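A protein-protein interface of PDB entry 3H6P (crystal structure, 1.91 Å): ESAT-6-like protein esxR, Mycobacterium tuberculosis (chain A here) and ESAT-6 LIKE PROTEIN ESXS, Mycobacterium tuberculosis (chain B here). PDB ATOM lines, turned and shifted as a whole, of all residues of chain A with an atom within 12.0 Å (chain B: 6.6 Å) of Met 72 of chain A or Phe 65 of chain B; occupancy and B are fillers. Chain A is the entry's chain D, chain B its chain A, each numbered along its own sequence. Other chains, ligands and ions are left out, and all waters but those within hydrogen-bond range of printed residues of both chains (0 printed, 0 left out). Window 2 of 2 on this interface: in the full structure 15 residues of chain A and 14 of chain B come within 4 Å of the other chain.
Among the printed residues, merely in contact across the chains: Leu 65 of chain A with Phe 72 of chain B (3.7 Å), Ala 68 of chain A with Ala 68 of chain B (3.5 Å), Ala 68 of chain A with Phe 72 of chain B (3.5 Å), Ser 71 of chain A with Ala 68 of chain B (3.7 Å), Met 72 of chain A with Phe 65 of chain B (3.5 Å), Met 72 of chain A with Ala 68 of chain B (3.7 Å), Met 72 of chain A with His 69 of chain B (3.4 Å) and Met 72 of chain A with Phe 72 of chain B (3.9 Å).
The backbone carbonyl oxygen (O) of Arg 67 of chain A sits at hydrogen-bond distance from the side-chain hydroxyl (OG) of Ser 71 of chain A (3.2 Å).
Hydrophobic or aromatic side chains of chain B within 4 Å of the printed part of chain A: Phe 65, Ala 68, His 69 and Phe 72. Of the 16 printed residues of chain A, 4 touch a printed residue of chain B. Along chain A the printed residues that touch a printed residue of chain B span positions 65 to 72.
Of the printed residues of chain B, Leu 65 of chain A touches Phe 72 (3.7 Å). Of the printed residues of chain B, Ala 68 of chain A touches Ala 68 and Phe 72. Of the printed residues of chain B, Ser 71 of chain A touches Ala 68. Met 72 of chain A touches just these residues of chain B: Phe 65, Ala 68, His 69 and Phe 72. Gly 74 of chain A touches none of the printed residues of chain B. No residue of chain A comes within 4 Å of Ser 61 of chain B. No residue of chain A comes within 4 Å of Ala 63 of chain B. Of chain A, only Met 72 (3.5 Å) comes within 4 Å of Phe 65 of chain B. No residue of chain A comes within 4 Å of Gln 66 of chain B. His 69 of chain B touches one residue of chain A. Printed residues of chain A within 4 Å of Phe 72 of chain B: Leu 65, Ala 68 and Met 72. Val 73 of chain B touches none of the printed residues of chain A.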
ATOM      1  N   TYR A  21      14.685 -23.716 -13.600  1.00  0.00           N
ATOM      2  CA  TYR A  21      15.329 -25.025 -13.511  1.00  0.00           C
ATOM      3  C   TYR A  21      16.841 -25.018 -13.634  1.00  0.00           C
ATOM      4  O   TYR A  21      17.475 -25.897 -13.070  1.00  0.00           O
ATOM      5  CB  TYR A  21      14.725 -26.028 -14.495  1.00  0.00           C
ATOM      6  CG  TYR A  21      13.345 -26.433 -14.071  1.00  0.00           C
ATOM      7  CD1 TYR A  21      13.138 -27.101 -12.873  1.00  0.00           C
ATOM      8  CD2 TYR A  21      12.248 -26.122 -14.846  1.00  0.00           C
ATOM      9  CE1 TYR A  21      11.871 -27.455 -12.470  1.00  0.00           C
ATOM     10  CE2 TYR A  21      10.988 -26.480 -14.458  1.00  0.00           C
ATOM     11  CZ  TYR A  21      10.799 -27.148 -13.275  1.00  0.00           C
ATOM     12  OH  TYR A  21       9.519 -27.484 -12.892  1.00  0.00           O
ATOM     13  N   ALA A  22      17.412 -24.060 -14.366  1.00  0.00           N
ATOM     14  CA  ALA A  22      18.862 -24.006 -14.515  1.00  0.00           C
ATOM     15  C   ALA A  22      19.557 -23.988 -13.155  1.00  0.00           C
ATOM     16  O   ALA A  22      20.458 -24.790 -12.906  1.00  0.00           O
ATOM     17  CB  ALA A  22      19.274 -22.806 -15.337  1.00  0.00           C
ATOM     18  N   LEU A  25      18.897 -27.339 -11.156  1.00  0.00           N
ATOM     19  CA  LEU A  25      19.742 -28.423 -11.658  1.00  0.00           C
ATOM     20  C   LEU A  25      21.194 -28.238 -11.166  1.00  0.00           C
ATOM     21  O   LEU A  25      21.842 -29.216 -10.760  1.00  0.00           O
ATOM     22  CB  LEU A  25      19.691 -28.506 -13.198  1.00  0.00           C
ATOM     23  CG  LEU A  25      18.390 -28.989 -13.854  1.00  0.00           C
ATOM     24  CD1 LEU A  25      18.425 -28.731 -15.359  1.00  0.00           C
ATOM     25  CD2 LEU A  25      18.148 -30.457 -13.581  1.00  0.00           C
ATOM     26  N   LEU A  62      26.702 -32.171 -16.062  1.00  0.00           N
ATOM     27  CA  LEU A  62      25.800 -31.136 -15.533  1.00  0.00           C
ATOM     28  C   LEU A  62      25.902 -29.846 -16.328  1.00  0.00           C
ATOM     29  O   LEU A  62      24.903 -29.192 -16.580  1.00  0.00           O
ATOM     30  CB  LEU A  62      26.137 -30.804 -14.094  1.00  0.00           C
ATOM     31  CG  LEU A  62      25.506 -31.646 -13.009  1.00  0.00           C
ATOM     32  CD1 LEU A  62      25.559 -33.109 -13.348  1.00  0.00           C
ATOM     33  CD2 LEU A  62      26.249 -31.345 -11.721  1.00  0.00           C
ATOM     34  N   GLU A  63      27.121 -29.476 -16.693  1.00  0.00           N
ATOM     35  CA  GLU A  63      27.338 -28.274 -17.480  1.00  0.00           C
ATOM     36  C   GLU A  63      26.608 -28.424 -18.791  1.00  0.00           C
ATOM     37  O   GLU A  63      25.852 -27.549 -19.194  1.00  0.00           O
ATOM     38  CB  GLU A  63      28.812 -28.092 -17.781  1.00  0.00           C
ATOM     39  CG  GLU A  63      29.628 -27.521 -16.666  1.00  0.00           C
ATOM     40  CD  GLU A  63      31.082 -27.413 -17.066  1.00  0.00           C
ATOM     41  OE1 GLU A  63      31.358 -26.726 -18.082  1.00  0.00           O
ATOM     42  OE2 GLU A  63      31.938 -28.026 -16.378  1.00  0.00           O
ATOM     43  N   ASP A  64      26.838 -29.551 -19.450  1.00  0.00           N
ATOM     44  CA  ASP A  64      26.215 -29.819 -20.738  1.00  0.00           C
ATOM     45  C   ASP A  64      24.699 -29.814 -20.637  1.00  0.00           C
ATOM     46  O   ASP A  64      24.022 -29.307 -21.524  1.00  0.00           O
ATOM     47  CB  ASP A  64      26.681 -31.167 -21.294  1.00  0.00           C
ATOM     48  CG  ASP A  64      28.160 -31.180 -21.667  1.00  0.00           C
ATOM     49  OD1 ASP A  64      28.820 -30.101 -21.666  1.00  0.00           O
ATOM     50  OD2 ASP A  64      28.655 -32.292 -21.964  1.00  0.00           O
ATOM     51  N   LEU A  65      24.180 -30.410 -19.560  1.00  0.00           N
ATOM     52  CA  LEU A  65      22.756 -30.516 -19.311  1.00  0.00           C
ATOM     53  C   LEU A  65      22.121 -29.135 -19.143  1.00  0.00           C
ATOM     54  O   LEU A  65      21.150 -28.806 -19.812  1.00  0.00           O
ATOM     55  CB  LEU A  65      22.511 -31.357 -18.049  1.00  0.00           C
ATOM     56  CG  LEU A  65      21.058 -31.693 -17.727  1.00  0.00           C
ATOM     57  CD1 LEU A  65      20.526 -32.846 -18.568  1.00  0.00           C
ATOM     58  CD2 LEU A  65      20.947 -32.011 -16.241  1.00  0.00           C
ATOM     59  N   VAL A  66      22.675 -28.341 -18.240  1.00  0.00           N
ATOM     60  CA  VAL A  66      22.178 -26.995 -17.969  1.00  0.00           C
ATOM     61  C   VAL A  66      22.298 -26.062 -19.190  1.00  0.00           C
ATOM     62  O   VAL A  66      21.376 -25.308 -19.482  1.00  0.00           O
ATOM     63  CB  VAL A  66      22.909 -26.367 -16.752  1.00  0.00           C
ATOM     64  CG1 VAL A  66      22.529 -24.903 -16.597  1.00  0.00           C
ATOM     65  CG2 VAL A  66      22.581 -27.156 -15.487  1.00  0.00           C
ATOM     66  N   ARG A  67      23.407 -26.127 -19.920  1.00  0.00           N
ATOM     67  CA  ARG A  67      23.569 -25.283 -21.120  1.00  0.00           C
ATOM     68  C   ARG A  67      22.551 -25.638 -22.215  1.00  0.00           C
ATOM     69  O   ARG A  67      21.991 -24.751 -22.854  1.00  0.00           O
ATOM     70  CB  ARG A  67      24.990 -25.383 -21.666  1.00  0.00           C
ATOM     71  CG  ARG A  67      26.030 -24.741 -20.771  1.00  0.00           C
ATOM     72  CD  ARG A  67      27.416 -24.802 -21.397  1.00  0.00           C
ATOM     73  NE  ARG A  67      28.393 -24.027 -20.623  1.00  0.00           N
ATOM     74  CZ  ARG A  67      28.625 -22.717 -20.751  1.00  0.00           C
ATOM     75  NH1 ARG A  67      27.966 -21.971 -21.644  1.00  0.00           N
ATOM     76  NH2 ARG A  67      29.546 -22.139 -19.978  1.00  0.00           N
ATOM     77  N   ALA A  68      22.304 -26.930 -22.416  1.00  0.00           N
ATOM     78  CA  ALA A  68      21.263 -27.380 -23.351  1.00  0.00           C
ATOM     79  C   ALA A  68      19.853 -26.921 -22.936  1.00  0.00           C
ATOM     80  O   ALA A  68      19.049 -26.518 -23.774  1.00  0.00           O
ATOM     81  CB  ALA A  68      21.305 -28.901 -23.499  1.00  0.00           C
ATOM     82  N   TYR A  69      19.559 -26.972 -21.643  1.00  0.00           N
ATOM     83  CA  TYR A  69      18.258 -26.523 -21.121  1.00  0.00           C
ATOM     84  C   TYR A  69      18.015 -25.017 -21.381  1.00  0.00           C
ATOM     85  O   TYR A  69      16.919 -24.588 -21.797  1.00  0.00           O
ATOM     86  CB  TYR A  69      18.165 -26.799 -19.615  1.00  0.00           C
ATOM     87  CG  TYR A  69      17.019 -26.080 -18.998  1.00  0.00           C
ATOM     88  CD1 TYR A  69      15.722 -26.550 -19.146  1.00  0.00           C
ATOM     89  CD2 TYR A  69      17.211 -24.873 -18.327  1.00  0.00           C
ATOM     90  CE1 TYR A  69      14.637 -25.852 -18.618  1.00  0.00           C
ATOM     91  CE2 TYR A  69      16.123 -24.170 -17.793  1.00  0.00           C
ATOM     92  CZ  TYR A  69      14.843 -24.668 -17.942  1.00  0.00           C
ATOM     93  OH  TYR A  69      13.774 -23.960 -17.402  1.00  0.00           O
ATOM     94  N   GLN A  70      19.038 -24.224 -21.097  1.00  0.00           N
ATOM     95  CA  GLN A  70      19.002 -22.788 -21.345  1.00  0.00           C
ATOM     96  C   GLN A  70      18.847 -22.467 -22.822  1.00  0.00           C
ATOM     97  O   GLN A  70      18.170 -21.496 -23.169  1.00  0.00           O
ATOM     98  CB  GLN A  70      20.260 -22.124 -20.789  1.00  0.00           C
ATOM     99  CG  GLN A  70      20.256 -22.093 -19.263  1.00  0.00           C
ATOM    100  CD  GLN A  70      21.542 -21.569 -18.660  1.00  0.00           C
ATOM    101  OE1 GLN A  70      22.641 -21.917 -19.097  1.00  0.00           O
ATOM    102  NE2 GLN A  70      21.412 -20.756 -17.620  1.00  0.00           N
ATOM    103  N   SER A  71      19.458 -23.269 -23.692  1.00  0.00           N
ATOM    104  CA  SER A  71      19.284 -23.085 -25.142  1.00  0.00           C
ATOM    105  C   SER A  71      17.861 -23.443 -25.584  1.00  0.00           C
ATOM    106  O   SER A  71      17.250 -22.705 -26.372  1.00  0.00           O
ATOM    107  CB  SER A  71      20.294 -23.913 -25.929  1.00  0.00           C
ATOM    108  OG  SER A  71      21.601 -23.427 -25.716  1.00  0.00           O
ATOM    109  N   MET A  72      17.340 -24.562 -25.074  1.00  0.00           N
ATOM    110  CA  MET A  72      15.963 -24.997 -25.364  1.00  0.00           C
ATOM    111  C   MET A  72      14.932 -23.952 -24.963  1.00  0.00           C
ATOM    112  O   MET A  72      13.991 -23.695 -25.704  1.00  0.00           O
ATOM    113  CB  MET A  72      15.608 -26.297 -24.603  1.00  0.00           C
ATOM    114  CG  MET A  72      16.168 -27.623 -25.144  1.00  0.00           C
ATOM    115  SD  MET A  72      15.770 -29.021 -24.039  1.00  0.00           S
ATOM    116  CE  MET A  72      14.144 -29.419 -24.601  1.00  0.00           C
ATOM    117  N   SER A  73      15.077 -23.383 -23.772  1.00  0.00           N
ATOM    118  CA  SER A  73      14.010 -22.536 -23.194  1.00  0.00           C
ATOM    119  C   SER A  73      14.205 -21.044 -23.418  1.00  0.00           C
ATOM    120  O   SER A  73      13.291 -20.267 -23.137  1.00  0.00           O
ATOM    121  CB  SER A  73      13.807 -22.833 -21.694  1.00  0.00           C
ATOM    122  OG  SER A  73      15.031 -22.784 -20.974  1.00  0.00           O
ATOM    123  N   GLY A  74      15.367 -20.636 -23.926  1.00  0.00           N
ATOM    124  CA  GLY A  74      15.631 -19.221 -24.162  1.00  0.00           C
ATOM    125  C   GLY A  74      17.107 -18.880 -24.279  1.00  0.00           C
ATOM    126  O   GLY A  74      17.471 -17.877 -24.907  1.00  0.00           O
ATOM    127  N   GLU B  60      15.296 -21.237 -38.014  1.00  0.00           N
ATOM    128  CA  GLU B  60      16.536 -21.232 -37.227  1.00  0.00           C
ATOM    129  C   GLU B  60      16.238 -21.571 -35.770  1.00  0.00           C
ATOM    130  O   GLU B  60      16.932 -22.361 -35.159  1.00  0.00           O
ATOM    131  CB  GLU B  60      17.221 -19.866 -37.297  1.00  0.00           C
ATOM    132  CG  GLU B  60      17.905 -19.515 -38.620  1.00  0.00           C
ATOM    133  CD  GLU B  60      18.973 -20.510 -39.081  1.00  0.00           C
ATOM    134  OE1 GLU B  60      20.182 -20.305 -38.762  1.00  0.00           O
ATOM    135  OE2 GLU B  60      18.609 -21.484 -39.796  1.00  0.00           O
ATOM    136  N   SER B  61      15.176 -20.994 -35.231  1.00  0.00           N
ATOM    137  CA  SER B  61      14.720 -21.305 -33.876  1.00  0.00           C
ATOM    138  C   SER B  61      14.356 -22.785 -33.719  1.00  0.00           C
ATOM    139  O   SER B  61      14.769 -23.451 -32.752  1.00  0.00           O
ATOM    140  CB  SER B  61      13.518 -20.403 -33.501  1.00  0.00           C
ATOM    141  OG  SER B  61      12.968 -20.826 -32.249  1.00  0.00           O
ATOM    142  N   ALA B  62      13.604 -23.312 -34.676  1.00  0.00           N
ATOM    143  CA  ALA B  62      13.180 -24.717 -34.640  1.00  0.00           C
ATOM    144  C   ALA B  62      14.391 -25.669 -34.689  1.00  0.00           C
ATOM    145  O   ALA B  62      14.509 -26.601 -33.879  1.00  0.00           O
ATOM    146  CB  ALA B  62      12.226 -24.993 -35.772  1.00  0.00           C
ATOM    147  N   ALA B  63      15.312 -25.395 -35.601  1.00  0.00           N
ATOM    148  CA  ALA B  63      16.557 -26.168 -35.715  1.00  0.00           C
ATOM    149  C   ALA B  63      17.428 -26.073 -34.461  1.00  0.00           C
ATOM    150  O   ALA B  63      18.002 -27.084 -34.034  1.00  0.00           O
ATOM    151  CB  ALA B  63      17.348 -25.691 -36.926  1.00  0.00           C
ATOM    152  N   ALA B  64      17.536 -24.874 -33.880  1.00  0.00           N
ATOM    153  CA  ALA B  64      18.356 -24.681 -32.674  1.00  0.00           C
ATOM    154  C   ALA B  64      17.720 -25.438 -31.502  1.00  0.00           C
ATOM    155  O   ALA B  64      18.414 -26.099 -30.735  1.00  0.00           O
ATOM    156  CB  ALA B  64      18.536 -23.200 -32.348  1.00  0.00           C
ATOM    157  N   PHE B  65      16.406 -25.382 -31.383  1.00  0.00           N
ATOM    158  CA  PHE B  65      15.725 -26.154 -30.347  1.00  0.00           C
ATOM    159  C   PHE B  65      15.936 -27.676 -30.476  1.00  0.00           C
ATOM    160  O   PHE B  65      16.184 -28.370 -29.482  1.00  0.00           O
ATOM    161  CB  PHE B  65      14.223 -25.877 -30.332  1.00  0.00           C
ATOM    162  CG  PHE B  65      13.506 -26.674 -29.299  1.00  0.00           C
ATOM    163  CD1 PHE B  65      13.563 -26.298 -27.972  1.00  0.00           C
ATOM    164  CD2 PHE B  65      12.813 -27.831 -29.643  1.00  0.00           C
ATOM    165  CE1 PHE B  65      12.937 -27.067 -26.999  1.00  0.00           C
ATOM    166  CE2 PHE B  65      12.186 -28.593 -28.680  1.00  0.00           C
ATOM    167  CZ  PHE B  65      12.247 -28.193 -27.358  1.00  0.00           C
ATOM    168  N   GLN B  66      15.807 -28.198 -31.683  1.00  0.00           N
ATOM    169  CA  GLN B  66      16.035 -29.632 -31.922  1.00  0.00           C
ATOM    170  C   GLN B  66      17.459 -30.045 -31.538  1.00  0.00           C
ATOM    171  O   GLN B  66      17.653 -31.061 -30.863  1.00  0.00           O
ATOM    172  CB  GLN B  66      15.756 -29.994 -33.382  1.00  0.00           C
ATOM    173  CG  GLN B  66      14.286 -30.018 -33.737  1.00  0.00           C
ATOM    174  N   GLY B  67      18.453 -29.251 -31.927  1.00  0.00           N
ATOM    175  CA  GLY B  67      19.839 -29.531 -31.518  1.00  0.00           C
ATOM    176  C   GLY B  67      20.044 -29.510 -30.008  1.00  0.00           C
ATOM    177  O   GLY B  67      20.618 -30.430 -29.429  1.00  0.00           O
ATOM    178  N   ALA B  68      19.568 -28.442 -29.375  1.00  0.00           N
ATOM    179  CA  ALA B  68      19.620 -28.292 -27.931  1.00  0.00           C
ATOM    180  C   ALA B  68      18.965 -29.479 -27.233  1.00  0.00           C
ATOM    181  O   ALA B  68      19.520 -30.025 -26.271  1.00  0.00           O
ATOM    182  CB  ALA B  68      18.938 -26.985 -27.517  1.00  0.00           C
ATOM    183  N   HIS B  69      17.788 -29.870 -27.719  1.00  0.00           N
ATOM    184  CA  HIS B  69      17.011 -30.967 -27.135  1.00  0.00           C
ATOM    185  C   HIS B  69      17.752 -32.295 -27.219  1.00  0.00           C
ATOM    186  O   HIS B  69      17.790 -33.058 -26.246  1.00  0.00           O
ATOM    187  CB  HIS B  69      15.631 -31.067 -27.798  1.00  0.00           C
ATOM    188  CG  HIS B  69      14.688 -32.004 -27.105  1.00  0.00           C
ATOM    189  ND1 HIS B  69      13.528 -32.457 -27.689  1.00  0.00           N
ATOM    190  CD2 HIS B  69      14.720 -32.550 -25.866  1.00  0.00           C
ATOM    191  CE1 HIS B  69      12.899 -33.262 -26.850  1.00  0.00           C
ATOM    192  NE2 HIS B  69      13.604 -33.334 -25.735  1.00  0.00           N
ATOM    193  N   ALA B  70      18.345 -32.565 -28.373  1.00  0.00           N
ATOM    194  CA  ALA B  70      19.220 -33.712 -28.551  1.00  0.00           C
ATOM    195  C   ALA B  70      20.397 -33.688 -27.556  1.00  0.00           C
ATOM    196  O   ALA B  70      20.702 -34.712 -26.933  1.00  0.00           O
ATOM    197  CB  ALA B  70      19.715 -33.767 -30.022  1.00  0.00           C
ATOM    198  N   PHE B  72      20.539 -32.109 -24.675  1.00  0.00           N
ATOM    199  CA  PHE B  72      19.952 -32.288 -23.345  1.00  0.00           C
ATOM    200  C   PHE B  72      19.709 -33.779 -23.018  1.00  0.00           C
ATOM    201  O   PHE B  72      20.050 -34.259 -21.932  1.00  0.00           O
ATOM    202  CB  PHE B  72      18.631 -31.495 -23.253  1.00  0.00           C
ATOM    203  CG  PHE B  72      17.939 -31.612 -21.910  1.00  0.00           C
ATOM    204  CD1 PHE B  72      18.133 -30.661 -20.927  1.00  0.00           C
ATOM    205  CD2 PHE B  72      17.099 -32.674 -21.639  1.00  0.00           C
ATOM    206  CE1 PHE B  72      17.481 -30.775 -19.675  1.00  0.00           C
ATOM    207  CE2 PHE B  72      16.465 -32.791 -20.399  1.00  0.00           C
ATOM    208  CZ  PHE B  72      16.646 -31.835 -19.438  1.00  0.00           C
ATOM    209  N   VAL B  73      19.099 -34.489 -23.959  1.00  0.00           N
ATOM    210  CA  VAL B  73      18.834 -35.921 -23.831  1.00  0.00           C
ATOM    211  C   VAL B  73      20.152 -36.706 -23.668  1.00  0.00           C
ATOM    212  O   VAL B  73      20.258 -37.556 -22.782  1.00  0.00           O
ATOM    213  CB  VAL B  73      17.982 -36.407 -25.019  1.00  0.00           C
ATOM    214  CG1 VAL B  73      17.921 -37.925 -25.105  1.00  0.00           C
ATOM    215  CG2 VAL B  73      16.584 -35.815 -24.905  1.00  0.00           C
